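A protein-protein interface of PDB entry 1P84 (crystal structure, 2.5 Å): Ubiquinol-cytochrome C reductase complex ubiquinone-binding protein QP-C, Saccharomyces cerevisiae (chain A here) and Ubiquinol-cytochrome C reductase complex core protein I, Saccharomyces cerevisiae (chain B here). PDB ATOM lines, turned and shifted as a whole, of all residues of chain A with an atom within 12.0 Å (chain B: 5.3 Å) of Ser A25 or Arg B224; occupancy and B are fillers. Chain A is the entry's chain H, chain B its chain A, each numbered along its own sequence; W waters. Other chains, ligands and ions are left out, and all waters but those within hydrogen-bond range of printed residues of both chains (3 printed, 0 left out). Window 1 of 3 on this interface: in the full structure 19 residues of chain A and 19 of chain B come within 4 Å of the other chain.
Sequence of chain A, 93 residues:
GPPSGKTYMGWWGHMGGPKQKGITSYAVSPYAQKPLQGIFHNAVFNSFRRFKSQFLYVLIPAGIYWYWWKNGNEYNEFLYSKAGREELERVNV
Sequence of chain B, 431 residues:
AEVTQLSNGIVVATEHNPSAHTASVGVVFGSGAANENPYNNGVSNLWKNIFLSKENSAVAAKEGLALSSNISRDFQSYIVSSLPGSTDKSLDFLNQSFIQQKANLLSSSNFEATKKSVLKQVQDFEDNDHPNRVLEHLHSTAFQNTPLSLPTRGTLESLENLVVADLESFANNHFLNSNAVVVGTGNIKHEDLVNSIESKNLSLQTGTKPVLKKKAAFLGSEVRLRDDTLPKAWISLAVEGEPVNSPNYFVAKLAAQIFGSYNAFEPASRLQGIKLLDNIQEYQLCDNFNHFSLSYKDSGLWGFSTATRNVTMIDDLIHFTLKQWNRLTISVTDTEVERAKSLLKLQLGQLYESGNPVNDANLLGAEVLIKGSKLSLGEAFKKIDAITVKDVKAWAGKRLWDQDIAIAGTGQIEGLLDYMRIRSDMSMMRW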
ATOM      1  N   TRP A  12       5.600  15.632  27.834  1.00  0.00           N
ATOM      2  CA  TRP A  12       4.293  16.111  27.393  1.00  0.00           C
ATOM      3  C   TRP A  12       4.183  17.643  27.372  1.00  0.00           C
ATOM      4  O   TRP A  12       4.348  18.309  28.401  1.00  0.00           O
ATOM      5  CB  TRP A  12       3.201  15.529  28.294  1.00  0.00           C
ATOM      6  CG  TRP A  12       3.234  14.038  28.354  1.00  0.00           C
ATOM      7  CD1 TRP A  12       3.677  13.272  29.390  1.00  0.00           C
ATOM      8  CD2 TRP A  12       2.837  13.128  27.324  1.00  0.00           C
ATOM      9  NE1 TRP A  12       3.584  11.942  29.071  1.00  0.00           N
ATOM     10  CE2 TRP A  12       3.069  11.824  27.807  1.00  0.00           C
ATOM     11  CE3 TRP A  12       2.305  13.286  26.038  1.00  0.00           C
ATOM     12  CZ2 TRP A  12       2.785  10.676  27.045  1.00  0.00           C
ATOM     13  CZ3 TRP A  12       2.021  12.149  25.279  1.00  0.00           C
ATOM     14  CH2 TRP A  12       2.261  10.862  25.787  1.00  0.00           C
ATOM     15  N   GLY A  13       3.935  18.191  26.182  1.00  0.00           N
ATOM     16  CA  GLY A  13       3.818  19.629  26.033  1.00  0.00           C
ATOM     17  C   GLY A  13       5.046  20.273  25.416  1.00  0.00           C
ATOM     18  O   GLY A  13       4.987  21.411  24.963  1.00  0.00           O
ATOM     19  N   MET A  15       7.724  17.907  23.822  1.00  0.00           N
ATOM     20  CA  MET A  15       8.389  16.676  23.419  1.00  0.00           C
ATOM     21  C   MET A  15       9.628  16.862  22.553  1.00  0.00           C
ATOM     22  O   MET A  15      10.502  15.989  22.533  1.00  0.00           O
ATOM     23  CB  MET A  15       7.398  15.763  22.703  1.00  0.00           C
ATOM     24  CG  MET A  15       7.722  14.289  22.809  1.00  0.00           C
ATOM     25  SD  MET A  15       7.524  13.708  24.486  1.00  0.00           S
ATOM     26  CE  MET A  15       5.696  13.584  24.590  1.00  0.00           C
ATOM     27  N   GLN A  20       3.285  20.966  14.691  1.00  0.00           N
ATOM     28  CA  GLN A  20       2.288  20.271  13.890  1.00  0.00           C
ATOM     29  C   GLN A  20       1.103  21.176  13.599  1.00  0.00           C
ATOM     30  O   GLN A  20       0.711  21.970  14.437  1.00  0.00           O
ATOM     31  CB  GLN A  20       1.814  19.015  14.623  1.00  0.00           C
ATOM     32  CG  GLN A  20       2.923  18.046  14.997  1.00  0.00           C
ATOM     33  CD  GLN A  20       2.386  16.768  15.610  1.00  0.00           C
ATOM     34  OE1 GLN A  20       1.213  16.425  15.431  1.00  0.00           O
ATOM     35  NE2 GLN A  20       3.239  16.052  16.340  1.00  0.00           N
ATOM     36  N   LYS A  21       0.517  21.022  12.418  1.00  0.00           N
ATOM     37  CA  LYS A  21      -0.625  21.823  11.980  1.00  0.00           C
ATOM     38  C   LYS A  21      -1.243  21.089  10.788  1.00  0.00           C
ATOM     39  O   LYS A  21      -0.537  20.421  10.037  1.00  0.00           O
ATOM     40  CB  LYS A  21      -0.133  23.207  11.530  1.00  0.00           C
ATOM     41  CG  LYS A  21      -1.194  24.298  11.443  1.00  0.00           C
ATOM     42  CD  LYS A  21      -0.596  25.582  10.841  1.00  0.00           C
ATOM     43  CE  LYS A  21      -1.443  26.835  11.106  1.00  0.00           C
ATOM     44  NZ  LYS A  21      -2.873  26.679  10.702  1.00  0.00           N
ATOM     45  N   GLY A  22      -2.560  21.162  10.652  1.00  0.00           N
ATOM     46  CA  GLY A  22      -3.225  20.514   9.536  1.00  0.00           C
ATOM     47  C   GLY A  22      -3.640  19.069   9.728  1.00  0.00           C
ATOM     48  O   GLY A  22      -4.498  18.569   8.988  1.00  0.00           O
ATOM     49  N   ILE A  23      -3.019  18.385  10.689  1.00  0.00           N
ATOM     50  CA  ILE A  23      -3.335  16.982  10.969  1.00  0.00           C
ATOM     51  C   ILE A  23      -4.460  16.872  11.999  1.00  0.00           C
ATOM     52  O   ILE A  23      -4.412  17.507  13.051  1.00  0.00           O
ATOM     53  CB  ILE A  23      -2.101  16.238  11.503  1.00  0.00           C
ATOM     54  CG1 ILE A  23      -0.929  16.421  10.540  1.00  0.00           C
ATOM     55  CG2 ILE A  23      -2.415  14.757  11.678  1.00  0.00           C
ATOM     56  CD1 ILE A  23       0.420  16.333  11.208  1.00  0.00           C
ATOM     57  N   THR A  24      -5.440  16.023  11.709  1.00  0.00           N
ATOM     58  CA  THR A  24      -6.583  15.827  12.585  1.00  0.00           C
ATOM     59  C   THR A  24      -6.811  14.344  12.882  1.00  0.00           C
ATOM     60  O   THR A  24      -7.019  13.550  11.970  1.00  0.00           O
ATOM     61  CB  THR A  24      -7.858  16.435  11.931  1.00  0.00           C
ATOM     62  OG1 THR A  24      -7.695  17.852  11.813  1.00  0.00           O
ATOM     63  CG2 THR A  24      -9.113  16.138  12.756  1.00  0.00           C
ATOM     64  N   SER A  25      -6.793  13.970  14.159  1.00  0.00           N
ATOM     65  CA  SER A  25      -6.994  12.572  14.533  1.00  0.00           C
ATOM     66  C   SER A  25      -8.387  12.335  15.073  1.00  0.00           C
ATOM     67  O   SER A  25      -9.011  13.246  15.612  1.00  0.00           O
ATOM     68  CB  SER A  25      -5.933  12.101  15.545  1.00  0.00           C
ATOM     69  OG  SER A  25      -5.914  12.884  16.732  1.00  0.00           O
ATOM     70  N   TYR A  26      -8.868  11.110  14.890  1.00  0.00           N
ATOM     71  CA  TYR A  26     -10.192  10.696  15.339  1.00  0.00           C
ATOM     72  C   TYR A  26     -10.087   9.327  15.990  1.00  0.00           C
ATOM     73  O   TYR A  26      -9.332   8.471  15.521  1.00  0.00           O
ATOM     74  CB  TYR A  26     -11.149  10.549  14.153  1.00  0.00           C
ATOM     75  CG  TYR A  26     -11.437  11.805  13.367  1.00  0.00           C
ATOM     76  CD1 TYR A  26     -10.563  12.248  12.373  1.00  0.00           C
ATOM     77  CD2 TYR A  26     -12.627  12.512  13.558  1.00  0.00           C
ATOM     78  CE1 TYR A  26     -10.874  13.357  11.588  1.00  0.00           C
ATOM     79  CE2 TYR A  26     -12.944  13.619  12.773  1.00  0.00           C
ATOM     80  CZ  TYR A  26     -12.068  14.033  11.792  1.00  0.00           C
ATOM     81  OH  TYR A  26     -12.394  15.111  11.003  1.00  0.00           O
ATOM     82  N   ALA A  27     -10.885   9.093  17.025  1.00  0.00           N
ATOM     83  CA  ALA A  27     -10.876   7.800  17.692  1.00  0.00           C
ATOM     84  C   ALA A  27     -12.222   7.513  18.327  1.00  0.00           C
ATOM     85  O   ALA A  27     -12.996   8.422  18.600  1.00  0.00           O
ATOM     86  CB  ALA A  27      -9.762   7.736  18.738  1.00  0.00           C
ATOM     87  N   VAL A  28     -12.480   6.236  18.562  1.00  0.00           N
ATOM     88  CA  VAL A  28     -13.720   5.776  19.158  1.00  0.00           C
ATOM     89  C   VAL A  28     -13.396   4.959  20.402  1.00  0.00           C
ATOM     90  O   VAL A  28     -12.474   4.139  20.390  1.00  0.00           O
ATOM     91  CB  VAL A  28     -14.512   4.912  18.135  1.00  0.00           C
ATOM     92  CG1 VAL A  28     -15.561   4.051  18.829  1.00  0.00           C
ATOM     93  CG2 VAL A  28     -15.176   5.823  17.112  1.00  0.00           C
ATOM     94  N   SER A  29     -14.151   5.188  21.474  1.00  0.00           N
ATOM     95  CA  SER A  29     -13.943   4.476  22.727  1.00  0.00           C
ATOM     96  C   SER A  29     -13.945   2.964  22.564  1.00  0.00           C
ATOM     97  O   SER A  29     -14.736   2.423  21.795  1.00  0.00           O
ATOM     98  CB  SER A  29     -15.022   4.851  23.743  1.00  0.00           C
ATOM     99  OG  SER A  29     -14.968   3.998  24.883  1.00  0.00           O
ATOM    100  N   PRO A  30     -13.026   2.268  23.261  1.00  0.00           N
ATOM    101  CA  PRO A  30     -12.904   0.809  23.225  1.00  0.00           C
ATOM    102  C   PRO A  30     -14.189   0.200  23.757  1.00  0.00           C
ATOM    103  O   PRO A  30     -14.531  -0.939  23.453  1.00  0.00           O
ATOM    104  CB  PRO A  30     -11.758   0.548  24.199  1.00  0.00           C
ATOM    105  CG  PRO A  30     -10.895   1.736  24.007  1.00  0.00           C
ATOM    106  CD  PRO A  30     -11.892   2.862  23.988  1.00  0.00           C
ATOM    107  N   GLU B 222     -13.548  10.968  20.097  1.00  0.00           N
ATOM    108  CA  GLU B 222     -12.791  12.211  20.163  1.00  0.00           C
ATOM    109  C   GLU B 222     -12.307  12.681  18.798  1.00  0.00           C
ATOM    110  O   GLU B 222     -12.204  11.900  17.857  1.00  0.00           O
ATOM    111  CB  GLU B 222     -11.569  12.017  21.053  1.00  0.00           C
ATOM    112  CG  GLU B 222     -10.541  11.035  20.478  1.00  0.00           C
ATOM    113  CD  GLU B 222      -9.378  10.756  21.423  1.00  0.00           C
ATOM    114  OE1 GLU B 222      -8.241  10.613  20.940  1.00  0.00           O
ATOM    115  OE2 GLU B 222      -9.602  10.659  22.647  1.00  0.00           O
ATOM    116  N   VAL B 223     -12.000  13.970  18.718  1.00  0.00           N
ATOM    117  CA  VAL B 223     -11.475  14.583  17.513  1.00  0.00           C
ATOM    118  C   VAL B 223     -10.434  15.587  18.007  1.00  0.00           C
ATOM    119  O   VAL B 223     -10.730  16.494  18.786  1.00  0.00           O
ATOM    120  CB  VAL B 223     -12.584  15.253  16.640  1.00  0.00           C
ATOM    121  CG1 VAL B 223     -13.398  16.264  17.444  1.00  0.00           C
ATOM    122  CG2 VAL B 223     -11.960  15.919  15.421  1.00  0.00           C
ATOM    123  N   ARG B 224      -9.193  15.373  17.598  1.00  0.00           N
ATOM    124  CA  ARG B 224      -8.096  16.225  18.023  1.00  0.00           C
ATOM    125  C   ARG B 224      -7.573  17.054  16.858  1.00  0.00           C
ATOM    126  O   ARG B 224      -7.074  16.514  15.870  1.00  0.00           O
ATOM    127  CB  ARG B 224      -7.001  15.354  18.663  1.00  0.00           C
ATOM    128  CG  ARG B 224      -7.560  14.420  19.756  1.00  0.00           C
ATOM    129  CD  ARG B 224      -6.588  13.321  20.183  1.00  0.00           C
ATOM    130  NE  ARG B 224      -5.880  13.660  21.411  1.00  0.00           N
ATOM    131  CZ  ARG B 224      -6.178  13.188  22.623  1.00  0.00           C
ATOM    132  NH1 ARG B 224      -5.462  13.582  23.659  1.00  0.00           N
ATOM    133  NH2 ARG B 224      -7.177  12.328  22.810  1.00  0.00           N
ATOM    134  N   LEU B 225      -7.746  18.367  16.969  1.00  0.00           N
ATOM    135  CA  LEU B 225      -7.331  19.321  15.941  1.00  0.00           C
ATOM    136  C   LEU B 225      -6.062  20.042  16.355  1.00  0.00           C
ATOM    137  O   LEU B 225      -6.043  21.269  16.461  1.00  0.00           O
ATOM    138  CB  LEU B 225      -8.457  20.334  15.716  1.00  0.00           C
ATOM    139  CG  LEU B 225      -9.756  19.775  15.107  1.00  0.00           C
ATOM    140  CD1 LEU B 225     -10.978  20.247  15.861  1.00  0.00           C
ATOM    141  CD2 LEU B 225      -9.841  20.188  13.658  1.00  0.00           C
ATOM    142  N   ARG B 226      -4.988  19.285  16.554  1.00  0.00           N
ATOM    143  CA  ARG B 226      -3.726  19.877  16.991  1.00  0.00           C
ATOM    144  C   ARG B 226      -3.262  20.992  16.071  1.00  0.00           C
ATOM    145  O   ARG B 226      -3.392  20.900  14.859  1.00  0.00           O
ATOM    146  CB  ARG B 226      -2.627  18.810  17.113  1.00  0.00           C
ATOM    147  CG  ARG B 226      -1.644  19.077  18.258  1.00  0.00           C
ATOM    148  CD  ARG B 226      -0.184  18.879  17.867  1.00  0.00           C
ATOM    149  NE  ARG B 226       0.440  17.720  18.506  1.00  0.00           N
ATOM    150  CZ  ARG B 226       1.700  17.680  18.940  1.00  0.00           C
ATOM    151  NH1 ARG B 226       2.164  16.570  19.490  1.00  0.00           N
ATOM    152  NH2 ARG B 226       2.496  18.737  18.841  1.00  0.00           N
ATOM    153  N   ILE B 407     -14.539  14.063  23.466  1.00  0.00           N
ATOM    154  CA  ILE B 407     -13.515  15.096  23.609  1.00  0.00           C
ATOM    155  C   ILE B 407     -13.265  15.791  22.275  1.00  0.00           C
ATOM    156  O   ILE B 407     -13.489  15.215  21.218  1.00  0.00           O
ATOM    157  CB  ILE B 407     -12.148  14.479  24.117  1.00  0.00           C
ATOM    158  CG1 ILE B 407     -12.385  13.596  25.338  1.00  0.00           C
ATOM    159  CG2 ILE B 407     -11.160  15.580  24.501  1.00  0.00           C
ATOM    160  CD1 ILE B 407     -11.165  12.876  25.812  1.00  0.00           C
ATOM    161  N   GLY B 409     -10.534  19.252  20.808  1.00  0.00           N
ATOM    162  CA  GLY B 409      -9.652  20.340  21.172  1.00  0.00           C
ATOM    163  C   GLY B 409      -8.802  20.819  20.019  1.00  0.00           C
ATOM    164  O   GLY B 409      -8.671  20.131  19.013  1.00  0.00           O
ATOM    165  N   ILE B 413      -2.318  21.027  22.061  1.00  0.00           N
ATOM    166  CA  ILE B 413      -2.855  19.901  22.834  1.00  0.00           C
ATOM    167  C   ILE B 413      -1.998  18.623  22.923  1.00  0.00           C
ATOM    168  O   ILE B 413      -2.532  17.517  23.098  1.00  0.00           O
ATOM    169  CB  ILE B 413      -4.275  19.503  22.360  1.00  0.00           C
ATOM    170  CG1 ILE B 413      -4.278  19.189  20.864  1.00  0.00           C
ATOM    171  CG2 ILE B 413      -5.263  20.613  22.661  1.00  0.00           C
ATOM    172  CD1 ILE B 413      -5.580  18.578  20.367  1.00  0.00           C
ATOM    173  N   LEU B 416      -2.493  16.839  26.274  1.00  0.00           N
ATOM    174  CA  LEU B 416      -3.769  16.201  26.589  1.00  0.00           C
ATOM    175  C   LEU B 416      -3.558  14.711  26.352  1.00  0.00           C
ATOM    176  O   LEU B 416      -3.385  14.279  25.220  1.00  0.00           O
ATOM    177  CB  LEU B 416      -4.872  16.751  25.675  1.00  0.00           C
ATOM    178  CG  LEU B 416      -6.289  16.185  25.816  1.00  0.00           C
ATOM    179  CD1 LEU B 416      -6.961  16.701  27.078  1.00  0.00           C
ATOM    180  CD2 LEU B 416      -7.100  16.578  24.609  1.00  0.00           C
ATOM    181  N   LEU B 417      -3.512  13.930  27.421  1.00  0.00           N
ATOM    182  CA  LEU B 417      -3.274  12.488  27.304  1.00  0.00           C
ATOM    183  C   LEU B 417      -4.275  11.719  26.444  1.00  0.00           C
ATOM    184  O   LEU B 417      -5.257  12.274  25.973  1.00  0.00           O
ATOM    185  CB  LEU B 417      -3.161  11.862  28.699  1.00  0.00           C
ATOM    186  CG  LEU B 417      -1.773  11.781  29.345  1.00  0.00           C
ATOM    187  CD1 LEU B 417      -0.898  12.940  28.928  1.00  0.00           C
ATOM    188  CD2 LEU B 417      -1.891  11.700  30.856  1.00  0.00           C
ATOM    189  N   ASP B 418      -4.008  10.436  26.244  1.00  0.00           N
ATOM    190  CA  ASP B 418      -4.858   9.562  25.436  1.00  0.00           C
ATOM    191  C   ASP B 418      -6.281   9.400  25.978  1.00  0.00           C
ATOM    192  O   ASP B 418      -6.546   9.684  27.137  1.00  0.00           O
ATOM    193  CB  ASP B 418      -4.213   8.189  25.341  1.00  0.00           C
ATOM    194  CG  ASP B 418      -4.023   7.562  26.694  1.00  0.00           C
ATOM    195  OD1 ASP B 418      -3.195   8.086  27.465  1.00  0.00           O
ATOM    196  OD2 ASP B 418      -4.731   6.583  27.004  1.00  0.00           O
ATOM    197  N   TYR B 419      -7.164   8.839  25.155  1.00  0.00           N
ATOM    198  CA  TYR B 419      -8.554   8.649  25.538  1.00  0.00           C
ATOM    199  C   TYR B 419      -8.731   7.837  26.804  1.00  0.00           C
ATOM    200  O   TYR B 419      -9.378   8.301  27.741  1.00  0.00           O
ATOM    201  CB  TYR B 419      -9.352   8.011  24.400  1.00  0.00           C
ATOM    202  CG  TYR B 419     -10.849   7.938  24.667  1.00  0.00           C
ATOM    203  CD1 TYR B 419     -11.682   9.023  24.375  1.00  0.00           C
ATOM    204  CD2 TYR B 419     -11.433   6.781  25.219  1.00  0.00           C
ATOM    205  CE1 TYR B 419     -13.059   8.965  24.625  1.00  0.00           C
ATOM    206  CE2 TYR B 419     -12.801   6.710  25.471  1.00  0.00           C
ATOM    207  CZ  TYR B 419     -13.610   7.810  25.170  1.00  0.00           C
ATOM    208  OH  TYR B 419     -14.969   7.761  25.406  1.00  0.00           O
HETATM  209  O   HOH W   1      -7.128  10.364  18.428  1.00  0.00           O
HETATM  210  O   HOH W   2      -1.883  19.115  13.422  1.00  0.00           O
HETATM  211  O   HOH W   3     -14.315  10.247  16.312  1.00  0.00           O
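O of Ala A27 is in hydrogen-bond range of N of Glu B222 (3.0 Å). The backbone NH of Arg B224 sits at hydrogen-bond distance from the backbone carbonyl oxygen of Ser A25 (2.9 Å). NE2 of Gln A20 sits close to NH1 of Arg B226, at 3.4 Å.
The side-chain carboxylate (OE1) of Glu B222 lies within salt-bridge range of the guanidinium group (NH2) of Arg B224 (2.8 Å). O of Ile B407 is in hydrogen-bond range of N of Val B223, 3.2 Å away. N of Gly B409 lies within hydrogen-bond range of O of Val B223. The backbone carbonyl oxygen (O) of Leu B416 is in hydrogen-bond range of the guanidinium group (NH1) of Arg B224, at 2.7 Å. The backbone carbonyl oxygen (O) of Leu B417 lies within hydrogen-bond range of the guanidinium group (NH1) of Arg B224. The backbone NH (N) of Leu B225 sits at hydrogen-bond distance from the backbone carbonyl oxygen (O) of Gly B409, 2.9 Å away.
Among the printed residues, merely in contact across the chains: Ser A29 with Tyr B419, Ser A25 with Val B223, Thr A24 with Arg B224, Tyr A26 with Glu B222, Tyr A26 with Val B223, Thr A24 with Leu B225, Thr A24 with Val B223 and Ile A23 with Arg B226.
Ser A25 touches two residues of chain B. Printed residues of chain B within 4 Å of Tyr A26: Glu B222 (3.4 Å) and Val B223 (3.6 Å). Glu B222 touches just these residues of chain A: Tyr A26 and Ala A27. Val B223 touches just these residues of chain A: Thr A24, Ser A25 and Tyr A26. Printed residues of chain A within 4 Å of Arg B224: Thr A24 and Ser A25. Of the printed residues of chain A, Arg B226 touches Gln A20 and Ile A23. No residue of chain A comes within 4 Å of Ile B407. No residue of chain A comes within 4 Å of Asp B418. Of the printed residues of chain A, Tyr B419 touches Ser A29. The nearest printed residue of chain A that does not touch Arg B224 is Ile A23 (4.002 Å). The nearest printed residue of chain B that does not touch Ser A29 is Glu B222 (6.0 Å).
Of the 14 printed residues of chain A, 7 touch a printed residue of chain B. Hydrophobic or aromatic side chains of chain A that line the printed part of chain B: Tyr A26 and Ala A27. Hydrophobic or aromatic side chains of chain B within 4 Å of the printed part of chain A: Val B223, Leu B225 and Tyr B419. Among the printed residues, 11 pairs touch across the chains.
Water W2 lies within hydrogen-bond range of the backbone carbonyl oxygen of Arg B226, the backbone carbonyl oxygen of Ile A23 and the backbone NH of Lys A21. Water W1 bridges OE1 of Glu B222 (2.8 Å) and OG of Ser A25 (3.3 Å). Water W3 lies within hydrogen-bond range of O of Glu B222 (3.1 Å) and O of Ala A27 (3.2 Å).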
